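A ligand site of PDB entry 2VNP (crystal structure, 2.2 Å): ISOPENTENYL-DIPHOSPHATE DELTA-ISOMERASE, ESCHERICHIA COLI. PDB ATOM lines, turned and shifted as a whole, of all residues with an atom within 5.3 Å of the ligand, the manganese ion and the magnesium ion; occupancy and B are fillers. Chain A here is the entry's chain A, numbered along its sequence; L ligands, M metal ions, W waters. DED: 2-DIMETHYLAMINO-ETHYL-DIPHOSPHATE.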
ATOM      1  N   GLU A   4       2.903  17.220  -0.767  1.00  0.00           N
ATOM      2  CA  GLU A   4       3.176  16.958   0.667  1.00  0.00           C
ATOM      3  C   GLU A   4       2.413  15.812   1.326  1.00  0.00           C
ATOM      4  O   GLU A   4       1.251  15.555   1.037  1.00  0.00           O
ATOM      5  CB  GLU A   4       2.976  18.225   1.489  1.00  0.00           C
ATOM      6  CG  GLU A   4       4.231  19.079   1.512  1.00  0.00           C
ATOM      7  CD  GLU A   4       4.161  20.292   2.425  1.00  0.00           C
ATOM      8  OE1 GLU A   4       4.591  21.348   1.888  1.00  0.00           O
ATOM      9  OE2 GLU A   4       3.766  20.204   3.647  1.00  0.00           O
ATOM     10  N   VAL A   6       2.136  13.347   5.296  1.00  0.00           N
ATOM     11  CA  VAL A   6       2.474  13.217   6.681  1.00  0.00           C
ATOM     12  C   VAL A   6       2.961  11.792   6.870  1.00  0.00           C
ATOM     13  O   VAL A   6       2.531  10.884   6.188  1.00  0.00           O
ATOM     14  CB  VAL A   6       1.288  13.552   7.670  1.00  0.00           C
ATOM     15  CG1 VAL A   6       0.860  15.004   7.543  1.00  0.00           C
ATOM     16  CG2 VAL A   6       0.111  12.603   7.550  1.00  0.00           C
ATOM     17  N   LYS A  21      -0.936  15.026   2.826  1.00  0.00           N
ATOM     18  CA  LYS A  21      -1.144  15.969   3.969  1.00  0.00           C
ATOM     19  C   LYS A  21      -2.568  16.514   4.193  1.00  0.00           C
ATOM     20  O   LYS A  21      -3.142  16.353   5.271  1.00  0.00           O
ATOM     21  CB  LYS A  21      -0.107  17.112   3.907  1.00  0.00           C
ATOM     22  CG  LYS A  21      -0.002  17.928   5.219  1.00  0.00           C
ATOM     23  CD  LYS A  21       1.073  19.037   5.101  1.00  0.00           C
ATOM     24  CE  LYS A  21       0.493  20.274   4.399  1.00  0.00           C
ATOM     25  NZ  LYS A  21       1.527  21.313   4.273  1.00  0.00           N
ATOM     26  N   HIS A  25      -5.943  15.064   7.272  1.00  0.00           N
ATOM     27  CA  HIS A  25      -6.587  15.787   8.423  1.00  0.00           C
ATOM     28  C   HIS A  25      -8.070  15.855   8.283  1.00  0.00           C
ATOM     29  O   HIS A  25      -8.579  16.500   7.380  1.00  0.00           O
ATOM     30  CB  HIS A  25      -6.004  17.198   8.603  1.00  0.00           C
ATOM     31  CG  HIS A  25      -4.538  17.177   8.920  1.00  0.00           C
ATOM     32  ND1 HIS A  25      -3.560  17.077   7.953  1.00  0.00           N
ATOM     33  CD2 HIS A  25      -3.889  17.170  10.110  1.00  0.00           C
ATOM     34  CE1 HIS A  25      -2.376  17.071   8.522  1.00  0.00           C
ATOM     35  NE2 HIS A  25      -2.547  17.110   9.827  1.00  0.00           N
ATOM     36  N   HIS A  32       0.203  11.039  13.603  1.00  0.00           N
ATOM     37  CA  HIS A  32       1.252  11.262  12.593  1.00  0.00           C
ATOM     38  C   HIS A  32       2.304  12.229  13.089  1.00  0.00           C
ATOM     39  O   HIS A  32       2.163  12.820  14.194  1.00  0.00           O
ATOM     40  CB  HIS A  32       0.641  11.732  11.254  1.00  0.00           C
ATOM     41  CG  HIS A  32      -0.045  13.067  11.330  1.00  0.00           C
ATOM     42  ND1 HIS A  32      -1.360  13.208  11.719  1.00  0.00           N
ATOM     43  CD2 HIS A  32       0.420  14.317  11.083  1.00  0.00           C
ATOM     44  CE1 HIS A  32      -1.684  14.484  11.711  1.00  0.00           C
ATOM     45  NE2 HIS A  32      -0.640  15.171  11.297  1.00  0.00           N
ATOM     46  N   ALA A  34       4.639  15.579  13.288  1.00  0.00           N
ATOM     47  CA  ALA A  34       4.523  17.029  13.148  1.00  0.00           C
ATOM     48  C   ALA A  34       5.738  17.635  13.888  1.00  0.00           C
ATOM     49  O   ALA A  34       6.526  16.876  14.439  1.00  0.00           O
ATOM     50  CB  ALA A  34       3.199  17.492  13.723  1.00  0.00           C
ATOM     51  N   PHE A  35       5.895  18.974  13.875  1.00  0.00           N
ATOM     52  CA  PHE A  35       6.822  19.702  14.812  1.00  0.00           C
ATOM     53  C   PHE A  35       6.157  21.019  15.185  1.00  0.00           C
ATOM     54  O   PHE A  35       5.344  21.493  14.445  1.00  0.00           O
ATOM     55  CB  PHE A  35       8.197  20.001  14.164  1.00  0.00           C
ATOM     56  CG  PHE A  35       8.107  21.001  13.003  1.00  0.00           C
ATOM     57  CD1 PHE A  35       8.051  22.359  13.236  1.00  0.00           C
ATOM     58  CD2 PHE A  35       7.970  20.557  11.697  1.00  0.00           C
ATOM     59  CE1 PHE A  35       7.883  23.256  12.168  1.00  0.00           C
ATOM     60  CE2 PHE A  35       7.808  21.474  10.617  1.00  0.00           C
ATOM     61  CZ  PHE A  35       7.754  22.786  10.854  1.00  0.00           C
ATOM     62  N   SER A  36       6.563  21.645  16.287  1.00  0.00           N
ATOM     63  CA  SER A  36       6.282  23.046  16.579  1.00  0.00           C
ATOM     64  C   SER A  36       7.587  23.696  16.914  1.00  0.00           C
ATOM     65  O   SER A  36       8.491  23.033  17.455  1.00  0.00           O
ATOM     66  CB  SER A  36       5.357  23.226  17.756  1.00  0.00           C
ATOM     67  OG  SER A  36       4.141  22.580  17.439  1.00  0.00           O
ATOM     68  N   ARG A  51      -2.744  32.018  12.193  1.00  0.00           N
ATOM     69  CA  ARG A  51      -2.821  31.210  10.953  1.00  0.00           C
ATOM     70  C   ARG A  51      -3.821  31.805   9.928  1.00  0.00           C
ATOM     71  O   ARG A  51      -4.870  32.348  10.368  1.00  0.00           O
ATOM     72  CB  ARG A  51      -3.296  29.855  11.332  1.00  0.00           C
ATOM     73  CG  ARG A  51      -2.438  29.192  12.402  1.00  0.00           C
ATOM     74  CD  ARG A  51      -3.053  27.871  12.941  1.00  0.00           C
ATOM     75  NE  ARG A  51      -3.536  26.817  11.993  1.00  0.00           N
ATOM     76  CZ  ARG A  51      -2.740  25.922  11.383  1.00  0.00           C
ATOM     77  NH1 ARG A  51      -1.417  25.955  11.550  1.00  0.00           N
ATOM     78  NH2 ARG A  51      -3.263  24.957  10.630  1.00  0.00           N
ATOM     79  N   LYS A  55      -6.295  28.156   6.099  1.00  0.00           N
ATOM     80  CA  LYS A  55      -5.794  26.894   6.665  1.00  0.00           C
ATOM     81  C   LYS A  55      -6.991  26.059   6.902  1.00  0.00           C
ATOM     82  O   LYS A  55      -8.021  26.576   7.290  1.00  0.00           O
ATOM     83  CB  LYS A  55      -4.979  27.052   7.984  1.00  0.00           C
ATOM     84  CG  LYS A  55      -3.798  27.998   7.917  1.00  0.00           C
ATOM     85  CD  LYS A  55      -2.699  27.547   6.906  1.00  0.00           C
ATOM     86  CE  LYS A  55      -2.146  26.126   7.214  1.00  0.00           C
ATOM     87  NZ  LYS A  55      -0.955  25.822   6.305  1.00  0.00           N
ATOM     88  N   ALA A  57      -7.125  23.350   9.112  1.00  0.00           N
ATOM     89  CA  ALA A  57      -7.313  23.134  10.512  1.00  0.00           C
ATOM     90  C   ALA A  57      -6.964  24.426  11.340  1.00  0.00           C
ATOM     91  O   ALA A  57      -5.948  25.093  11.090  1.00  0.00           O
ATOM     92  CB  ALA A  57      -6.533  21.920  10.994  1.00  0.00           C
ATOM     93  N   VAL A  66       5.935  28.804  14.223  1.00  0.00           N
ATOM     94  CA  VAL A  66       5.858  27.936  13.055  1.00  0.00           C
ATOM     95  C   VAL A  66       5.783  26.474  13.414  1.00  0.00           C
ATOM     96  O   VAL A  66       6.598  25.973  14.219  1.00  0.00           O
ATOM     97  CB  VAL A  66       6.833  28.265  11.835  1.00  0.00           C
ATOM     98  CG1 VAL A  66       7.662  29.538  11.935  1.00  0.00           C
ATOM     99  CG2 VAL A  66       7.543  27.143  11.267  1.00  0.00           C
ATOM    100  N   CYS A  67       4.772  25.852  12.804  1.00  0.00           N
ATOM    101  CA  CYS A  67       4.478  24.431  12.961  1.00  0.00           C
ATOM    102  C   CYS A  67       4.285  23.863  11.586  1.00  0.00           C
ATOM    103  O   CYS A  67       3.983  24.598  10.600  1.00  0.00           O
ATOM    104  CB  CYS A  67       3.188  24.221  13.767  1.00  0.00           C
ATOM    105  SG  CYS A  67       3.194  24.960  15.413  1.00  0.00           S
ATOM    106  N   GLY A  68       4.418  22.537  11.517  1.00  0.00           N
ATOM    107  CA  GLY A  68       4.387  21.823  10.235  1.00  0.00           C
ATOM    108  C   GLY A  68       4.612  20.328  10.421  1.00  0.00           C
ATOM    109  O   GLY A  68       4.470  19.772  11.524  1.00  0.00           O
ATOM    110  N   HIS A  69       4.935  19.684   9.300  1.00  0.00           N
ATOM    111  CA  HIS A  69       4.813  18.212   9.158  1.00  0.00           C
ATOM    112  C   HIS A  69       6.109  17.797   8.424  1.00  0.00           C
ATOM    113  O   HIS A  69       6.297  18.203   7.278  1.00  0.00           O
ATOM    114  CB  HIS A  69       3.566  17.844   8.309  1.00  0.00           C
ATOM    115  CG  HIS A  69       2.234  18.039   9.005  1.00  0.00           C
ATOM    116  ND1 HIS A  69       1.358  19.067   8.692  1.00  0.00           N
ATOM    117  CD2 HIS A  69       1.628  17.318   9.986  1.00  0.00           C
ATOM    118  CE1 HIS A  69       0.291  18.981   9.466  1.00  0.00           C
ATOM    119  NE2 HIS A  69       0.410  17.899  10.226  1.00  0.00           N
ATOM    120  N   ARG A  83      10.012  25.299   6.840  1.00  0.00           N
ATOM    121  CA  ARG A  83       8.721  26.015   7.074  1.00  0.00           C
ATOM    122  C   ARG A  83       8.892  27.496   7.479  1.00  0.00           C
ATOM    123  O   ARG A  83       8.070  28.325   7.092  1.00  0.00           O
ATOM    124  CB  ARG A  83       7.753  25.256   8.032  1.00  0.00           C
ATOM    125  CG  ARG A  83       7.179  23.925   7.477  1.00  0.00           C
ATOM    126  CD  ARG A  83       6.595  24.073   6.040  1.00  0.00           C
ATOM    127  NE  ARG A  83       5.232  24.628   6.090  1.00  0.00           N
ATOM    128  CZ  ARG A  83       4.334  24.528   5.102  1.00  0.00           C
ATOM    129  NH1 ARG A  83       4.654  23.921   4.009  1.00  0.00           N
ATOM    130  NH2 ARG A  83       3.121  25.043   5.213  1.00  0.00           N
ATOM    131  N   GLU A  87       7.010  29.853   5.375  1.00  0.00           N
ATOM    132  CA  GLU A  87       5.849  30.636   5.949  1.00  0.00           C
ATOM    133  C   GLU A  87       6.160  32.106   6.268  1.00  0.00           C
ATOM    134  O   GLU A  87       5.308  33.014   6.167  1.00  0.00           O
ATOM    135  CB  GLU A  87       5.253  29.935   7.173  1.00  0.00           C
ATOM    136  CG  GLU A  87       4.853  28.511   6.947  1.00  0.00           C
ATOM    137  CD  GLU A  87       4.293  27.832   8.255  1.00  0.00           C
ATOM    138  OE1 GLU A  87       4.171  28.525   9.294  1.00  0.00           O
ATOM    139  OE2 GLU A  87       3.953  26.616   8.253  1.00  0.00           O
ATOM    140  N   TYR A 104      -0.325  14.978  21.200  1.00  0.00           N
ATOM    141  CA  TYR A 104      -1.663  15.482  21.583  1.00  0.00           C
ATOM    142  C   TYR A 104      -2.647  15.059  20.477  1.00  0.00           C
ATOM    143  O   TYR A 104      -2.241  14.679  19.343  1.00  0.00           O
ATOM    144  CB  TYR A 104      -1.618  17.016  21.708  1.00  0.00           C
ATOM    145  CG  TYR A 104      -1.667  17.702  20.360  1.00  0.00           C
ATOM    146  CD1 TYR A 104      -2.843  18.247  19.862  1.00  0.00           C
ATOM    147  CD2 TYR A 104      -0.519  17.734  19.559  1.00  0.00           C
ATOM    148  CE1 TYR A 104      -2.858  18.835  18.590  1.00  0.00           C
ATOM    149  CE2 TYR A 104      -0.518  18.313  18.356  1.00  0.00           C
ATOM    150  CZ  TYR A 104      -1.664  18.877  17.847  1.00  0.00           C
ATOM    151  OH  TYR A 104      -1.575  19.397  16.568  1.00  0.00           O
ATOM    152  N   GLU A 114      -6.438  17.281  14.828  1.00  0.00           N
ATOM    153  CA  GLU A 114      -5.036  17.017  14.763  1.00  0.00           C
ATOM    154  C   GLU A 114      -4.712  15.922  15.768  1.00  0.00           C
ATOM    155  O   GLU A 114      -5.287  15.852  16.876  1.00  0.00           O
ATOM    156  CB  GLU A 114      -4.230  18.271  14.954  1.00  0.00           C
ATOM    157  CG  GLU A 114      -3.966  19.068  13.647  1.00  0.00           C
ATOM    158  CD  GLU A 114      -2.806  18.490  12.829  1.00  0.00           C
ATOM    159  OE1 GLU A 114      -2.098  19.230  12.146  1.00  0.00           O
ATOM    160  OE2 GLU A 114      -2.546  17.272  12.864  1.00  0.00           O
ATOM    161  N   ASN A 115      -3.862  14.994  15.315  1.00  0.00           N
ATOM    162  CA  ASN A 115      -3.505  13.790  16.086  1.00  0.00           C
ATOM    163  C   ASN A 115      -2.036  13.619  15.827  1.00  0.00           C
ATOM    164  O   ASN A 115      -1.647  13.130  14.783  1.00  0.00           O
ATOM    165  CB  ASN A 115      -4.330  12.566  15.632  1.00  0.00           C
ATOM    166  CG  ASN A 115      -4.349  11.458  16.675  1.00  0.00           C
ATOM    167  OD1 ASN A 115      -3.868  11.622  17.831  1.00  0.00           O
ATOM    168  ND2 ASN A 115      -4.898  10.302  16.270  1.00  0.00           N
ATOM    169  N   GLU A 116      -1.198  14.123  16.719  1.00  0.00           N
ATOM    170  CA  GLU A 116       0.219  14.246  16.353  1.00  0.00           C
ATOM    171  C   GLU A 116       1.204  13.840  17.471  1.00  0.00           C
ATOM    172  O   GLU A 116       0.925  14.046  18.637  1.00  0.00           O
ATOM    173  CB  GLU A 116       0.566  15.647  15.840  1.00  0.00           C
ATOM    174  CG  GLU A 116      -0.203  16.067  14.621  1.00  0.00           C
ATOM    175  CD  GLU A 116       0.096  17.473  14.221  1.00  0.00           C
ATOM    176  OE1 GLU A 116       0.404  18.337  15.110  1.00  0.00           O
ATOM    177  OE2 GLU A 116       0.028  17.676  12.985  1.00  0.00           O
ATOM    178  N   CYS A 118       4.418  15.325  18.243  1.00  0.00           N
ATOM    179  CA  CYS A 118       4.751  16.673  17.836  1.00  0.00           C
ATOM    180  C   CYS A 118       5.925  17.260  18.630  1.00  0.00           C
ATOM    181  O   CYS A 118       5.726  18.236  19.403  1.00  0.00           O
ATOM    182  CB  CYS A 118       3.494  17.586  17.983  1.00  0.00           C
ATOM    183  SG  CYS A 118       3.653  19.311  17.269  1.00  0.00           S
ATOM    184  N   GLU A 135      -0.243  31.643   4.626  1.00  0.00           N
ATOM    185  CA  GLU A 135      -0.009  30.821   5.833  1.00  0.00           C
ATOM    186  C   GLU A 135      -0.323  31.609   7.066  1.00  0.00           C
ATOM    187  O   GLU A 135      -0.894  31.105   8.020  1.00  0.00           O
ATOM    188  CB  GLU A 135       1.437  30.296   5.860  1.00  0.00           C
ATOM    189  CG  GLU A 135       1.826  29.347   4.697  1.00  0.00           C
ATOM    190  CD  GLU A 135       1.082  28.009   4.733  1.00  0.00           C
ATOM    191  OE1 GLU A 135       0.785  27.455   5.843  1.00  0.00           O
ATOM    192  OE2 GLU A 135       0.750  27.506   3.619  1.00  0.00           O
ATOM    193  N   TRP A 161      -2.443  23.077  20.646  1.00  0.00           N
ATOM    194  CA  TRP A 161      -1.059  22.590  20.843  1.00  0.00           C
ATOM    195  C   TRP A 161      -0.186  23.669  21.485  1.00  0.00           C
ATOM    196  O   TRP A 161       0.618  23.387  22.361  1.00  0.00           O
ATOM    197  CB  TRP A 161      -0.410  22.058  19.596  1.00  0.00           C
ATOM    198  CG  TRP A 161      -0.425  23.027  18.453  1.00  0.00           C
ATOM    199  CD1 TRP A 161       0.512  23.933  18.180  1.00  0.00           C
ATOM    200  CD2 TRP A 161      -1.483  23.226  17.497  1.00  0.00           C
ATOM    201  NE1 TRP A 161       0.173  24.666  17.069  1.00  0.00           N
ATOM    202  CE2 TRP A 161      -1.049  24.251  16.618  1.00  0.00           C
ATOM    203  CE3 TRP A 161      -2.716  22.578  17.245  1.00  0.00           C
ATOM    204  CZ2 TRP A 161      -1.820  24.683  15.505  1.00  0.00           C
ATOM    205  CZ3 TRP A 161      -3.491  23.027  16.149  1.00  0.00           C
ATOM    206  CH2 TRP A 161      -3.037  24.090  15.314  1.00  0.00           C
HETATM  207  O1  DED L   1       2.181  21.570   7.110  1.00  0.00           O
HETATM  208  O2  DED L   1       2.147  24.041   7.695  1.00  0.00           O
HETATM  209  O3  DED L   1       0.065  22.881   6.845  1.00  0.00           O
HETATM  210  P4  DED L   1       1.330  22.769   7.602  1.00  0.00           P
HETATM  211  O5  DED L   1       0.769  22.296   9.059  1.00  0.00           O
HETATM  212  O6  DED L   1       0.854  24.441  10.358  1.00  0.00           O
HETATM  213  O7  DED L   1      -1.381  23.091  10.184  1.00  0.00           O
HETATM  214  P8  DED L   1       0.083  23.129  10.262  1.00  0.00           P
HETATM  215  O9  DED L   1       0.416  22.260  11.608  1.00  0.00           O
HETATM  216  C10 DED L   1       1.728  21.740  11.998  1.00  0.00           C
HETATM  217  C11 DED L   1       1.715  20.702  13.141  1.00  0.00           C
HETATM  218  N12 DED L   1       0.568  20.893  14.086  1.00  0.00           N
HETATM  219  C13 DED L   1       1.017  21.374  15.399  1.00  0.00           C
HETATM  220  C14 DED L   1      -0.638  21.612  13.692  1.00  0.00           C
HETATM  221 MN    MN M   1      -1.103  17.284  11.450  1.00  0.00          MN
HETATM  222 MG    MG M   2       2.530  25.584   9.397  1.00  0.00          MG
HETATM  223  O   HOH W   1      -2.047  21.386   6.209  1.00  0.00           O
HETATM  224  O   HOH W   2       1.000  27.255   8.510  1.00  0.00           O
HETATM  225  O   HOH W   3       2.588  27.090  11.084  1.00  0.00           O
HETATM  226  O   HOH W   4       4.883  21.286   7.020  1.00  0.00           O
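The side-chain carboxylate of Glu 116 lies within salt-bridge range of a nitrogen (N12) of the ligand, at 2.8 Å. N12 of the ligand lies close to OE1 of Glu 114 (3.7 Å). A ring nitrogen (ND1) of His 69 sits at hydrogen-bond distance from an oxygen (O1) of the ligand, at 3.1 Å. NH2 of Arg 51 lies within salt-bridge range of O7 of the ligand, at 2.7 Å. An oxygen (O2) of the ligand lies close to the guanidinium group of Arg 83, at 2.8 Å. The side-chain amino group (NZ) of Lys 21 lies within salt-bridge range of an oxygen (O1) of the ligand, 2.9 Å away. O3 of the ligand lies within salt-bridge range of NZ of Lys 55 (3.2 Å).
The side-chain hydroxyl (OH) of Tyr 104 lies within hydrogen-bond range of the side-chain carboxylate (OE1) of Glu 116 (2.7 Å). The side-chain sulfur of Cys 67 lies within hydrogen-bond range of the side-chain hydroxyl of Ser 36, at 3.3 Å. The backbone NH of His 32 lies within hydrogen-bond range of the backbone carbonyl oxygen of Asn 115, at 3.0 Å. A ring nitrogen (ND1) of His 25 is in hydrogen-bond range of the backbone carbonyl oxygen (O) of Lys 21. O of Gly 68 is in hydrogen-bond range of N of Phe 35 (2.9 Å). The guanidinium group (NH1) of Arg 83 lies within salt-bridge range of the side-chain carboxylate (OE1) of Glu 4 (3.3 Å). OE1 of Glu 135 is in salt-bridge range of NZ of Lys 55, at 2.4 Å. OG of Ser 36 sits at hydrogen-bond distance from SG of Cys 118 (3.3 Å).
Residues that only touch the ligand: Gly 68 (2.8 Å), Tyr 104 (3.5 Å), Ala 34 (3.6 Å), Trp 161 (3.7 Å), Cys 118 (3.8 Å), Ser 36 (3.9 Å) and Phe 35 (3.9 Å). The nearest printed residue that does not touch the ligand is Glu 4 (4.05 Å).
Within 4 Å of the manganese ion: His 25, His 32, His 69, Glu 114 and Glu 116. Along chain A the residues within 4 Å of the manganese ion span positions 25 to 116.
Of the 24 residues printed, 2 come within 4 Å of the magnesium ion. The nearest printed residue that does not touch the magnesium ion is Gly 68 (4.2 Å).
The manganese ion is bound by the side-chain carboxylate (OE2) of Glu 116, the side-chain carboxylate (OE2) of Glu 114, a ring nitrogen (NE2) of His 69, a ring nitrogen (NE2) of His 32, a ring nitrogen (NE2) of His 25 and the side-chain carboxylate (OE1) of Glu 114.
The side-chain carboxylate (OE2) of Glu 87 binds the magnesium ion, 2.1 Å away. The magnesium ion is bound by O of Cys 67, at 2.1 Å. The magnesium ion is bound by O6 of the ligand (2.2 Å). Water W3 binds the magnesium ion (2.3 Å). The magnesium ion is bound by an oxygen (O2) of the ligand (2.3 Å). The magnesium ion is bound by water W2.
Water W2 lies within hydrogen-bond range of OE1 of Glu 135 (2.7 Å) and NZ of Lys 55 (3.3 Å). Water W3 lies within hydrogen-bond range of OE1 of Glu 87 (2.8 Å) and N of Cys 67 (3.0 Å). Water W4 lies within hydrogen-bond range of O1 of the ligand (2.7 Å), N of His 69 (2.8 Å) and NE of Arg 83 (3.5 Å).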
